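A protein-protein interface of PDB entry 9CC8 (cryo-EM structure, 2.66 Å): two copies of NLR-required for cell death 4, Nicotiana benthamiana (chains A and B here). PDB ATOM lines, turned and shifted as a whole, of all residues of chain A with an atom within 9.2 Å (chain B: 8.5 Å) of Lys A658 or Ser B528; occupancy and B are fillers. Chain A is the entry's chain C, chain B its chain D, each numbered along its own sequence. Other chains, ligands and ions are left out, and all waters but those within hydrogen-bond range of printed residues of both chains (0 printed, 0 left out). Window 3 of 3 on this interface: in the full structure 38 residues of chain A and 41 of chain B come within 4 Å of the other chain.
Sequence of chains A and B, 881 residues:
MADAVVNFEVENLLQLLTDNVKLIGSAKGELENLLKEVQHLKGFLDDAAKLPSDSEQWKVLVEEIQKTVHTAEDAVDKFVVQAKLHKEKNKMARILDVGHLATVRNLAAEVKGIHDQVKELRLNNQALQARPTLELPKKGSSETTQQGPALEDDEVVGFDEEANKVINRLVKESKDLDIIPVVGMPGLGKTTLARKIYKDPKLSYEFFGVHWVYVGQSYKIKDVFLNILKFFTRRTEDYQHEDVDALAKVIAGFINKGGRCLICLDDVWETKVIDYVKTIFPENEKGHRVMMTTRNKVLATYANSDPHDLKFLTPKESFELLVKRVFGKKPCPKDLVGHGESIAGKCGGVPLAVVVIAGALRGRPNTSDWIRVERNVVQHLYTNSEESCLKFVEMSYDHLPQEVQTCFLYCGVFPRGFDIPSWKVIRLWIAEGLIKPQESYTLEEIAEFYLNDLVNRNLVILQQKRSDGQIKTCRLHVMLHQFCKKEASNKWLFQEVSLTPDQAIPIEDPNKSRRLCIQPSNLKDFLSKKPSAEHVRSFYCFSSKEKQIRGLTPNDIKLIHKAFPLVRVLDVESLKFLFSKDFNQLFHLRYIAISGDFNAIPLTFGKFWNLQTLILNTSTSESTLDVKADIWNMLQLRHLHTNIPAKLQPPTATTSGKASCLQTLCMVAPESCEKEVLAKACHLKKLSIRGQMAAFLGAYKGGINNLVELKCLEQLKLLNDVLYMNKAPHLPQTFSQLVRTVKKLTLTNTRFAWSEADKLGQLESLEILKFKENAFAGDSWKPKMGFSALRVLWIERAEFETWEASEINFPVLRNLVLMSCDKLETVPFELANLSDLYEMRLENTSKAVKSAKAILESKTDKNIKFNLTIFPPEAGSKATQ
His A683 touches Pro B501 (CD2 to CB, 3.5 Å).
NZ of Lys A658 is in hydrogen-bond range of OG of Ser B528, at 3.3 Å. SG of Cys A661 lies within hydrogen-bond range of OD2 of Asp B502 (3.4 Å). OD2 of Asp B502 lies close to O of Ala A659, at 3.0 Å.
No position is printed for both chains. Of the 4 pairs that touch across the chains among the printed residues, none has its exchanged pair printed and touching as well.
The backbone carbonyl oxygen (O) of Leu A635 sits close to the side-chain sulfur (SG) of Cys A661 (3.8 Å). The backbone carbonyl oxygen (O) of Lys A658 is in hydrogen-bond range of the side-chain amino group (NZ) of Lys A680, 2.9 Å away. The side-chain sulfur (SG) of Cys A682 is in hydrogen-bond range of a ring nitrogen (ND1) of His A683 (3.3 Å). The backbone carbonyl oxygen (O) of Asp B525 lies within hydrogen-bond range of the side-chain hydroxyl (OG) of Ser B528.
Of chain B, only Ser B528 (3.3 Å) comes within 4 Å of Lys A658. Of chain A, only Lys A658 comes within 4 Å of Ser B528. No residue of chain B comes within 4 Å of Gly A657. Ala A659 touches just one residue of chain B: Asp B502. Printed residues of chain A within 4 Å of Asp B502: Ala A659 (3.0 Å) and Cys A661 (3.4 Å). Printed residues of chain B within 4 Å of His A683: Pro B501 (3.5 Å). Of the printed residues of chain A, Pro B501 touches His A683. Of the printed residues of chain B, Cys A661 touches Asp B502. The nearest residue of chain B that does not touch Lys A658 is Asp B502 (4.3 Å).
Of the 20 printed residues of chain A, 4 touch a printed residue of chain B. Printed residues of chain A that touch a printed residue of chain B: Lys A658, Ala A659, Cys A661 and His A683. Of the 17 printed residues of chain B, 3 touch a printed residue of chain A. Among the printed residues, no Asp or Glu carboxylate lies within 4 Å of a Lys or Arg side-chain nitrogen of the other chain.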
ATOM      1  N   TRP A 632      -1.812  -2.819 -25.753  1.00  0.00           N
ATOM      2  CA  TRP A 632      -0.462  -2.270 -25.758  1.00  0.00           C
ATOM      3  C   TRP A 632       0.587  -3.349 -25.527  1.00  0.00           C
ATOM      4  O   TRP A 632       1.738  -3.190 -25.947  1.00  0.00           O
ATOM      5  CB  TRP A 632      -0.345  -1.171 -24.704  1.00  0.00           C
ATOM      6  CG  TRP A 632      -1.410  -0.142 -24.845  1.00  0.00           C
ATOM      7  CD1 TRP A 632      -2.359   0.185 -23.927  1.00  0.00           C
ATOM      8  CD2 TRP A 632      -1.658   0.680 -25.990  1.00  0.00           C
ATOM      9  NE1 TRP A 632      -3.178   1.169 -24.422  1.00  0.00           N
ATOM     10  CE2 TRP A 632      -2.769   1.490 -25.688  1.00  0.00           C
ATOM     11  CE3 TRP A 632      -1.047   0.813 -27.239  1.00  0.00           C
ATOM     12  CZ2 TRP A 632      -3.281   2.417 -26.587  1.00  0.00           C
ATOM     13  CZ3 TRP A 632      -1.556   1.735 -28.129  1.00  0.00           C
ATOM     14  CH2 TRP A 632      -2.661   2.525 -27.800  1.00  0.00           C
ATOM     15  N   ASN A 633       0.219  -4.443 -24.863  1.00  0.00           N
ATOM     16  CA  ASN A 633       1.125  -5.566 -24.670  1.00  0.00           C
ATOM     17  C   ASN A 633       1.040  -6.592 -25.789  1.00  0.00           C
ATOM     18  O   ASN A 633       1.793  -7.569 -25.769  1.00  0.00           O
ATOM     19  CB  ASN A 633       0.851  -6.255 -23.329  1.00  0.00           C
ATOM     20  CG  ASN A 633       1.250  -5.406 -22.127  1.00  0.00           C
ATOM     21  OD1 ASN A 633       0.748  -5.621 -21.028  1.00  0.00           O
ATOM     22  ND2 ASN A 633       2.153  -4.450 -22.325  1.00  0.00           N
ATOM     23  N   LEU A 635       2.402  -6.974 -28.789  1.00  0.00           N
ATOM     24  CA  LEU A 635       3.479  -6.316 -29.517  1.00  0.00           C
ATOM     25  C   LEU A 635       3.330  -6.488 -31.021  1.00  0.00           C
ATOM     26  O   LEU A 635       3.756  -5.619 -31.788  1.00  0.00           O
ATOM     27  CB  LEU A 635       4.835  -6.858 -29.060  1.00  0.00           C
ATOM     28  CG  LEU A 635       5.015  -7.151 -27.567  1.00  0.00           C
ATOM     29  CD1 LEU A 635       6.420  -7.662 -27.298  1.00  0.00           C
ATOM     30  CD2 LEU A 635       4.721  -5.918 -26.726  1.00  0.00           C
ATOM     31  N   PRO A 651      -2.258   3.072 -21.581  1.00  0.00           N
ATOM     32  CA  PRO A 651      -1.299   2.090 -21.066  1.00  0.00           C
ATOM     33  C   PRO A 651      -0.968   2.361 -19.607  1.00  0.00           C
ATOM     34  O   PRO A 651      -0.853   3.511 -19.177  1.00  0.00           O
ATOM     35  CB  PRO A 651      -0.074   2.277 -21.970  1.00  0.00           C
ATOM     36  CG  PRO A 651      -0.200   3.646 -22.507  1.00  0.00           C
ATOM     37  CD  PRO A 651      -1.667   3.917 -22.632  1.00  0.00           C
ATOM     38  N   THR A 654       3.241  -0.274 -16.098  1.00  0.00           N
ATOM     39  CA  THR A 654       3.907  -1.518 -16.465  1.00  0.00           C
ATOM     40  C   THR A 654       4.048  -1.642 -17.978  1.00  0.00           C
ATOM     41  O   THR A 654       5.095  -2.066 -18.480  1.00  0.00           O
ATOM     42  CB  THR A 654       3.131  -2.710 -15.908  1.00  0.00           C
ATOM     43  OG1 THR A 654       1.771  -2.650 -16.358  1.00  0.00           O
ATOM     44  CG2 THR A 654       3.157  -2.701 -14.386  1.00  0.00           C
ATOM     45  N   THR A 655       3.003  -1.272 -18.721  1.00  0.00           N
ATOM     46  CA  THR A 655       3.003  -1.422 -20.173  1.00  0.00           C
ATOM     47  C   THR A 655       3.934  -0.442 -20.870  1.00  0.00           C
ATOM     48  O   THR A 655       4.137  -0.569 -22.081  1.00  0.00           O
ATOM     49  CB  THR A 655       1.586  -1.247 -20.720  1.00  0.00           C
ATOM     50  OG1 THR A 655       1.139   0.090 -20.468  1.00  0.00           O
ATOM     51  CG2 THR A 655       0.630  -2.234 -20.068  1.00  0.00           C
ATOM     52  N   SER A 656       4.489   0.529 -20.150  1.00  0.00           N
ATOM     53  CA  SER A 656       5.418   1.469 -20.761  1.00  0.00           C
ATOM     54  C   SER A 656       6.625   0.729 -21.325  1.00  0.00           C
ATOM     55  O   SER A 656       7.114  -0.239 -20.737  1.00  0.00           O
ATOM     56  CB  SER A 656       5.868   2.509 -19.735  1.00  0.00           C
ATOM     57  OG  SER A 656       6.624   1.909 -18.698  1.00  0.00           O
ATOM     58  N   GLY A 657       7.099   1.187 -22.479  1.00  0.00           N
ATOM     59  CA  GLY A 657       8.245   0.574 -23.118  1.00  0.00           C
ATOM     60  C   GLY A 657       8.539   1.176 -24.476  1.00  0.00           C
ATOM     61  O   GLY A 657       8.590   2.401 -24.624  1.00  0.00           O
ATOM     62  N   LYS A 658       8.741   0.322 -25.475  1.00  0.00           N
ATOM     63  CA  LYS A 658       8.960   0.795 -26.830  1.00  0.00           C
ATOM     64  C   LYS A 658       7.645   1.286 -27.435  1.00  0.00           C
ATOM     65  O   LYS A 658       6.556   1.069 -26.896  1.00  0.00           O
ATOM     66  CB  LYS A 658       9.555  -0.316 -27.695  1.00  0.00           C
ATOM     67  CG  LYS A 658      10.750   0.115 -28.534  1.00  0.00           C
ATOM     68  CD  LYS A 658      11.622  -1.072 -28.920  1.00  0.00           C
ATOM     69  CE  LYS A 658      12.484  -1.551 -27.758  1.00  0.00           C
ATOM     70  NZ  LYS A 658      13.165  -2.837 -28.068  1.00  0.00           N
ATOM     71  N   ALA A 659       7.758   1.967 -28.571  1.00  0.00           N
ATOM     72  CA  ALA A 659       6.574   2.381 -29.307  1.00  0.00           C
ATOM     73  C   ALA A 659       5.840   1.157 -29.842  1.00  0.00           C
ATOM     74  O   ALA A 659       6.459   0.177 -30.264  1.00  0.00           O
ATOM     75  CB  ALA A 659       6.956   3.312 -30.456  1.00  0.00           C
ATOM     76  N   SER A 660       4.513   1.215 -29.810  1.00  0.00           N
ATOM     77  CA  SER A 660       3.706   0.111 -30.304  1.00  0.00           C
ATOM     78  C   SER A 660       3.835  -0.014 -31.817  1.00  0.00           C
ATOM     79  O   SER A 660       4.092   0.963 -32.526  1.00  0.00           O
ATOM     80  CB  SER A 660       2.241   0.307 -29.923  1.00  0.00           C
ATOM     81  OG  SER A 660       1.461  -0.799 -30.331  1.00  0.00           O
ATOM     82  N   CYS A 661       3.653  -1.240 -32.310  1.00  0.00           N
ATOM     83  CA  CYS A 661       3.698  -1.499 -33.744  1.00  0.00           C
ATOM     84  C   CYS A 661       2.456  -1.005 -34.472  1.00  0.00           C
ATOM     85  O   CYS A 661       2.420  -1.071 -35.704  1.00  0.00           O
ATOM     86  CB  CYS A 661       3.872  -2.997 -34.004  1.00  0.00           C
ATOM     87  SG  CYS A 661       5.565  -3.513 -34.343  1.00  0.00           S
ATOM     88  N   LEU A 662       1.451  -0.520 -33.750  1.00  0.00           N
ATOM     89  CA  LEU A 662       0.174  -0.162 -34.352  1.00  0.00           C
ATOM     90  C   LEU A 662       0.368   0.758 -35.548  1.00  0.00           C
ATOM     91  O   LEU A 662       1.040   1.787 -35.451  1.00  0.00           O
ATOM     92  CB  LEU A 662      -0.716   0.512 -33.307  1.00  0.00           C
ATOM     93  CG  LEU A 662      -1.914  -0.299 -32.819  1.00  0.00           C
ATOM     94  CD1 LEU A 662      -2.622   0.442 -31.700  1.00  0.00           C
ATOM     95  CD2 LEU A 662      -2.876  -0.592 -33.951  1.00  0.00           C
ATOM     96  N   GLU A 676      -0.935   9.419 -23.382  1.00  0.00           N
ATOM     97  CA  GLU A 676      -0.262   8.129 -23.284  1.00  0.00           C
ATOM     98  C   GLU A 676      -0.689   7.194 -24.408  1.00  0.00           C
ATOM     99  O   GLU A 676       0.147   6.483 -24.979  1.00  0.00           O
ATOM    100  CB  GLU A 676      -0.547   7.487 -21.926  1.00  0.00           C
ATOM    101  CG  GLU A 676      -0.520   8.454 -20.758  1.00  0.00           C
ATOM    102  CD  GLU A 676      -1.875   9.078 -20.488  1.00  0.00           C
ATOM    103  OE1 GLU A 676      -2.854   8.324 -20.305  1.00  0.00           O
ATOM    104  OE2 GLU A 676      -1.961  10.322 -20.466  1.00  0.00           O
ATOM    105  N   ALA A 679       1.051   8.471 -27.424  1.00  0.00           N
ATOM    106  CA  ALA A 679       2.495   8.306 -27.307  1.00  0.00           C
ATOM    107  C   ALA A 679       2.908   6.865 -27.569  1.00  0.00           C
ATOM    108  O   ALA A 679       3.886   6.615 -28.283  1.00  0.00           O
ATOM    109  CB  ALA A 679       2.961   8.752 -25.923  1.00  0.00           C
ATOM    110  N   LYS A 680       2.178   5.903 -26.999  1.00  0.00           N
ATOM    111  CA  LYS A 680       2.490   4.500 -27.249  1.00  0.00           C
ATOM    112  C   LYS A 680       2.318   4.149 -28.719  1.00  0.00           C
ATOM    113  O   LYS A 680       3.080   3.339 -29.258  1.00  0.00           O
ATOM    114  CB  LYS A 680       1.607   3.600 -26.385  1.00  0.00           C
ATOM    115  CG  LYS A 680       2.382   2.734 -25.409  1.00  0.00           C
ATOM    116  CD  LYS A 680       3.137   1.626 -26.122  1.00  0.00           C
ATOM    117  CE  LYS A 680       3.717   0.630 -25.135  1.00  0.00           C
ATOM    118  NZ  LYS A 680       4.350  -0.534 -25.807  1.00  0.00           N
ATOM    119  N   ALA A 681       1.331   4.748 -29.380  1.00  0.00           N
ATOM    120  CA  ALA A 681       1.052   4.514 -30.794  1.00  0.00           C
ATOM    121  C   ALA A 681       1.620   5.619 -31.674  1.00  0.00           C
ATOM    122  O   ALA A 681       1.005   6.008 -32.669  1.00  0.00           O
ATOM    123  CB  ALA A 681      -0.451   4.377 -31.012  1.00  0.00           C
ATOM    124  N   CYS A 682       2.796   6.149 -31.330  1.00  0.00           N
ATOM    125  CA  CYS A 682       3.352   7.268 -32.084  1.00  0.00           C
ATOM    126  C   CYS A 682       3.644   6.911 -33.536  1.00  0.00           C
ATOM    127  O   CYS A 682       3.782   7.814 -34.367  1.00  0.00           O
ATOM    128  CB  CYS A 682       4.627   7.778 -31.408  1.00  0.00           C
ATOM    129  SG  CYS A 682       5.722   6.486 -30.792  1.00  0.00           S
ATOM    130  N   HIS A 683       3.733   5.624 -33.868  1.00  0.00           N
ATOM    131  CA  HIS A 683       4.001   5.184 -35.230  1.00  0.00           C
ATOM    132  C   HIS A 683       2.724   4.983 -36.039  1.00  0.00           C
ATOM    133  O   HIS A 683       2.773   4.398 -37.126  1.00  0.00           O
ATOM    134  CB  HIS A 683       4.823   3.895 -35.210  1.00  0.00           C
ATOM    135  CG  HIS A 683       6.214   4.080 -34.687  1.00  0.00           C
ATOM    136  ND1 HIS A 683       6.503   4.882 -33.606  1.00  0.00           N
ATOM    137  CD2 HIS A 683       7.394   3.561 -35.098  1.00  0.00           C
ATOM    138  CE1 HIS A 683       7.802   4.850 -33.372  1.00  0.00           C
ATOM    139  NE2 HIS A 683       8.366   4.056 -34.263  1.00  0.00           N
ATOM    140  N   LYS A 711       4.346  10.504 -35.182  1.00  0.00           N
ATOM    141  CA  LYS A 711       5.491  10.871 -35.999  1.00  0.00           C
ATOM    142  C   LYS A 711       5.278  10.649 -37.485  1.00  0.00           C
ATOM    143  O   LYS A 711       5.909  11.335 -38.291  1.00  0.00           O
ATOM    144  CB  LYS A 711       6.725  10.077 -35.555  1.00  0.00           C
ATOM    145  CG  LYS A 711       7.099  10.292 -34.101  1.00  0.00           C
ATOM    146  CD  LYS A 711       8.273   9.421 -33.697  1.00  0.00           C
ATOM    147  CE  LYS A 711       8.711   9.701 -32.271  1.00  0.00           C
ATOM    148  NZ  LYS A 711       9.913   8.906 -31.897  1.00  0.00           N
ATOM    149  N   LEU B 499      17.000  -1.615 -38.211  1.00  0.00           N
ATOM    150  CA  LEU B 499      15.685  -1.889 -37.653  1.00  0.00           C
ATOM    151  C   LEU B 499      14.624  -1.066 -38.373  1.00  0.00           C
ATOM    152  O   LEU B 499      14.778   0.141 -38.572  1.00  0.00           O
ATOM    153  CB  LEU B 499      15.649  -1.564 -36.158  1.00  0.00           C
ATOM    154  CG  LEU B 499      16.920  -1.808 -35.339  1.00  0.00           C
ATOM    155  CD1 LEU B 499      16.739  -1.266 -33.934  1.00  0.00           C
ATOM    156  CD2 LEU B 499      17.263  -3.284 -35.287  1.00  0.00           C
ATOM    157  N   PRO B 501      11.155   0.507 -37.798  1.00  0.00           N
ATOM    158  CA  PRO B 501      10.709   0.854 -36.445  1.00  0.00           C
ATOM    159  C   PRO B 501      11.115  -0.157 -35.377  1.00  0.00           C
ATOM    160  O   PRO B 501      12.153   0.018 -34.731  1.00  0.00           O
ATOM    161  CB  PRO B 501       9.194   0.968 -36.638  1.00  0.00           C
ATOM    162  CG  PRO B 501       9.074   1.529 -38.100  1.00  0.00           C
ATOM    163  CD  PRO B 501      10.449   1.356 -38.766  1.00  0.00           C
ATOM    164  N   ASP B 502      10.326  -1.209 -35.181  1.00  0.00           N
ATOM    165  CA  ASP B 502      10.636  -2.253 -34.213  1.00  0.00           C
ATOM    166  C   ASP B 502      11.402  -3.375 -34.919  1.00  0.00           C
ATOM    167  O   ASP B 502      11.952  -3.178 -36.005  1.00  0.00           O
ATOM    168  CB  ASP B 502       9.345  -2.731 -33.541  1.00  0.00           C
ATOM    169  CG  ASP B 502       8.721  -1.664 -32.660  1.00  0.00           C
ATOM    170  OD1 ASP B 502       9.329  -0.584 -32.515  1.00  0.00           O
ATOM    171  OD2 ASP B 502       7.632  -1.908 -32.101  1.00  0.00           O
ATOM    172  N   GLN B 503      11.497  -4.548 -34.292  1.00  0.00           N
ATOM    173  CA  GLN B 503      12.072  -5.728 -34.931  1.00  0.00           C
ATOM    174  C   GLN B 503      13.590  -5.620 -35.012  1.00  0.00           C
ATOM    175  O   GLN B 503      14.193  -4.795 -34.317  1.00  0.00           O
ATOM    176  CB  GLN B 503      11.481  -5.934 -36.330  1.00  0.00           C
ATOM    177  CG  GLN B 503       9.962  -5.810 -36.404  1.00  0.00           C
ATOM    178  CD  GLN B 503       9.426  -6.074 -37.798  1.00  0.00           C
ATOM    179  OE1 GLN B 503      10.184  -6.106 -38.767  1.00  0.00           O
ATOM    180  NE2 GLN B 503       8.114  -6.244 -37.909  1.00  0.00           N
ATOM    181  N   ASN B 522      21.271   3.896 -34.101  1.00  0.00           N
ATOM    182  CA  ASN B 522      20.540   2.662 -33.844  1.00  0.00           C
ATOM    183  C   ASN B 522      21.097   1.870 -32.670  1.00  0.00           C
ATOM    184  O   ASN B 522      20.586   0.785 -32.379  1.00  0.00           O
ATOM    185  CB  ASN B 522      20.544   1.776 -35.092  1.00  0.00           C
ATOM    186  CG  ASN B 522      20.167   2.533 -36.344  1.00  0.00           C
ATOM    187  OD1 ASN B 522      20.742   2.316 -37.410  1.00  0.00           O
ATOM    188  ND2 ASN B 522      19.192   3.427 -36.224  1.00  0.00           N
ATOM    189  N   LEU B 523      22.131   2.374 -31.996  1.00  0.00           N
ATOM    190  CA  LEU B 523      22.743   1.614 -30.912  1.00  0.00           C
ATOM    191  C   LEU B 523      21.795   1.476 -29.727  1.00  0.00           C
ATOM    192  O   LEU B 523      21.609   0.375 -29.196  1.00  0.00           O
ATOM    193  CB  LEU B 523      24.048   2.283 -30.482  1.00  0.00           C
ATOM    194  CG  LEU B 523      24.815   1.585 -29.359  1.00  0.00           C
ATOM    195  CD1 LEU B 523      25.203   0.176 -29.767  1.00  0.00           C
ATOM    196  CD2 LEU B 523      26.040   2.396 -28.990  1.00  0.00           C
ATOM    197  N   LYS B 524      21.180   2.582 -29.301  1.00  0.00           N
ATOM    198  CA  LYS B 524      20.332   2.536 -28.114  1.00  0.00           C
ATOM    199  C   LYS B 524      19.171   1.569 -28.303  1.00  0.00           C
ATOM    200  O   LYS B 524      18.850   0.790 -27.400  1.00  0.00           O
ATOM    201  CB  LYS B 524      19.812   3.936 -27.786  1.00  0.00           C
ATOM    202  CG  LYS B 524      18.621   3.949 -26.836  1.00  0.00           C
ATOM    203  CD  LYS B 524      18.579   5.213 -25.984  1.00  0.00           C
ATOM    204  CE  LYS B 524      19.648   5.219 -24.899  1.00  0.00           C
ATOM    205  NZ  LYS B 524      19.671   3.967 -24.091  1.00  0.00           N
ATOM    206  N   ASP B 525      18.530   1.603 -29.471  1.00  0.00           N
ATOM    207  CA  ASP B 525      17.415   0.696 -29.722  1.00  0.00           C
ATOM    208  C   ASP B 525      17.877  -0.754 -29.719  1.00  0.00           C
ATOM    209  O   ASP B 525      17.189  -1.634 -29.189  1.00  0.00           O
ATOM    210  CB  ASP B 525      16.744   1.042 -31.051  1.00  0.00           C
ATOM    211  CG  ASP B 525      16.647   2.537 -31.284  1.00  0.00           C
ATOM    212  OD1 ASP B 525      16.764   2.966 -32.453  1.00  0.00           O
ATOM    213  OD2 ASP B 525      16.457   3.281 -30.299  1.00  0.00           O
ATOM    214  N   PHE B 526      19.039  -1.025 -30.316  1.00  0.00           N
ATOM    215  CA  PHE B 526      19.557  -2.388 -30.350  1.00  0.00           C
ATOM    216  C   PHE B 526      19.899  -2.883 -28.951  1.00  0.00           C
ATOM    217  O   PHE B 526      19.633  -4.043 -28.615  1.00  0.00           O
ATOM    218  CB  PHE B 526      20.779  -2.451 -31.262  1.00  0.00           C
ATOM    219  CG  PHE B 526      21.447  -3.794 -31.292  1.00  0.00           C
ATOM    220  CD1 PHE B 526      20.991  -4.790 -32.136  1.00  0.00           C
ATOM    221  CD2 PHE B 526      22.542  -4.055 -30.490  1.00  0.00           C
ATOM    222  CE1 PHE B 526      21.608  -6.023 -32.173  1.00  0.00           C
ATOM    223  CE2 PHE B 526      23.161  -5.288 -30.523  1.00  0.00           C
ATOM    224  CZ  PHE B 526      22.694  -6.271 -31.365  1.00  0.00           C
ATOM    225  N   LEU B 527      20.495  -2.025 -28.123  1.00  0.00           N
ATOM    226  CA  LEU B 527      20.879  -2.449 -26.783  1.00  0.00           C
ATOM    227  C   LEU B 527      19.666  -2.633 -25.881  1.00  0.00           C
ATOM    228  O   LEU B 527      19.690  -3.484 -24.985  1.00  0.00           O
ATOM    229  CB  LEU B 527      21.847  -1.439 -26.171  1.00  0.00           C
ATOM    230  CG  LEU B 527      23.277  -1.455 -26.718  1.00  0.00           C
ATOM    231  CD1 LEU B 527      24.116  -0.409 -26.010  1.00  0.00           C
ATOM    232  CD2 LEU B 527      23.911  -2.832 -26.583  1.00  0.00           C
ATOM    233  N   SER B 528      18.602  -1.855 -26.097  1.00  0.00           N
ATOM    234  CA  SER B 528      17.405  -1.998 -25.279  1.00  0.00           C
ATOM    235  C   SER B 528      16.821  -3.401 -25.369  1.00  0.00           C
ATOM    236  O   SER B 528      16.116  -3.828 -24.449  1.00  0.00           O
ATOM    237  CB  SER B 528      16.355  -0.972 -25.699  1.00  0.00           C
ATOM    238  OG  SER B 528      15.865  -1.248 -26.998  1.00  0.00           O
ATOM    239  N   LYS B 529      17.100  -4.123 -26.453  1.00  0.00           N
ATOM    240  CA  LYS B 529      16.695  -5.517 -26.571  1.00  0.00           C
ATOM    241  C   LYS B 529      17.530  -6.440 -25.694  1.00  0.00           C
ATOM    242  O   LYS B 529      17.219  -7.633 -25.609  1.00  0.00           O
ATOM    243  CB  LYS B 529      16.789  -5.954 -28.035  1.00  0.00           C
ATOM    244  CG  LYS B 529      16.064  -7.259 -28.363  1.00  0.00           C
ATOM    245  CD  LYS B 529      16.796  -8.076 -29.433  1.00  0.00           C
ATOM    246  CE  LYS B 529      18.135  -8.626 -28.949  1.00  0.00           C
ATOM    247  NZ  LYS B 529      18.047  -9.292 -27.621  1.00  0.00           N
ATOM    248  N   LYS B 530      18.578  -5.924 -25.050  1.00  0.00           N
ATOM    249  CA  LYS B 530      19.455  -6.739 -24.219  1.00  0.00           C
ATOM    250  C   LYS B 530      20.124  -7.800 -25.085  1.00  0.00           C
ATOM    251  O   LYS B 530      19.928  -9.003 -24.868  1.00  0.00           O
ATOM    252  CB  LYS B 530      18.668  -7.379 -23.073  1.00  0.00           C
ATOM    253  CG  LYS B 530      17.833  -6.384 -22.281  1.00  0.00           C
ATOM    254  CD  LYS B 530      17.142  -7.041 -21.102  1.00  0.00           C
ATOM    255  CE  LYS B 530      16.314  -6.036 -20.318  1.00  0.00           C
ATOM    256  NZ  LYS B 530      15.624  -6.663 -19.159  1.00  0.00           N
ATOM    257  N   PRO B 531      20.917  -7.389 -26.074  1.00  0.00           N
ATOM    258  CA  PRO B 531      21.495  -8.359 -27.009  1.00  0.00           C
ATOM    259  C   PRO B 531      22.425  -9.339 -26.312  1.00  0.00           C
ATOM    260  O   PRO B 531      23.139  -8.990 -25.370  1.00  0.00           O
ATOM    261  CB  PRO B 531      22.256  -7.476 -28.005  1.00  0.00           C
ATOM    262  CG  PRO B 531      22.540  -6.223 -27.259  1.00  0.00           C
ATOM    263  CD  PRO B 531      21.374  -6.018 -26.347  1.00  0.00           C
ATOM    264  N   LEU B 552      23.892   7.800 -24.728  1.00  0.00           N
ATOM    265  CA  LEU B 552      24.228   6.462 -24.260  1.00  0.00           C
ATOM    266  C   LEU B 552      24.707   6.548 -22.818  1.00  0.00           C
ATOM    267  O   LEU B 552      25.582   7.361 -22.500  1.00  0.00           O
ATOM    268  CB  LEU B 552      25.306   5.828 -25.140  1.00  0.00           C
ATOM    269  CG  LEU B 552      24.817   5.119 -26.405  1.00  0.00           C
ATOM    270  CD1 LEU B 552      24.190   3.779 -26.063  1.00  0.00           C
ATOM    271  CD2 LEU B 552      23.836   5.993 -27.166  1.00  0.00           C
ATOM    272  N   ASP B 556      24.406   1.205 -20.903  1.00  0.00           N
ATOM    273  CA  ASP B 556      24.484   0.793 -22.301  1.00  0.00           C
ATOM    274  C   ASP B 556      25.869   0.259 -22.644  1.00  0.00           C
ATOM    275  O   ASP B 556      25.997  -0.733 -23.369  1.00  0.00           O
ATOM    276  CB  ASP B 556      24.115   1.963 -23.211  1.00  0.00           C
ATOM    277  CG  ASP B 556      22.719   2.489 -22.945  1.00  0.00           C
ATOM    278  OD1 ASP B 556      21.788   1.666 -22.819  1.00  0.00           O
ATOM    279  OD2 ASP B 556      22.554   3.725 -22.862  1.00  0.00           O
ATOM    280  N   LEU B 559      26.120  -3.107 -21.259  1.00  0.00           N
ATOM    281  CA  LEU B 559      25.374  -4.026 -22.112  1.00  0.00           C
ATOM    282  C   LEU B 559      26.175  -4.393 -23.353  1.00  0.00           C
ATOM    283  O   LEU B 559      26.130  -5.538 -23.813  1.00  0.00           O
ATOM    284  CB  LEU B 559      24.035  -3.406 -22.506  1.00  0.00           C
ATOM    285  CG  LEU B 559      22.933  -3.452 -21.448  1.00  0.00           C
ATOM    286  CD1 LEU B 559      21.729  -2.650 -21.914  1.00  0.00           C
ATOM    287  CD2 LEU B 559      22.532  -4.885 -21.135  1.00  0.00           C
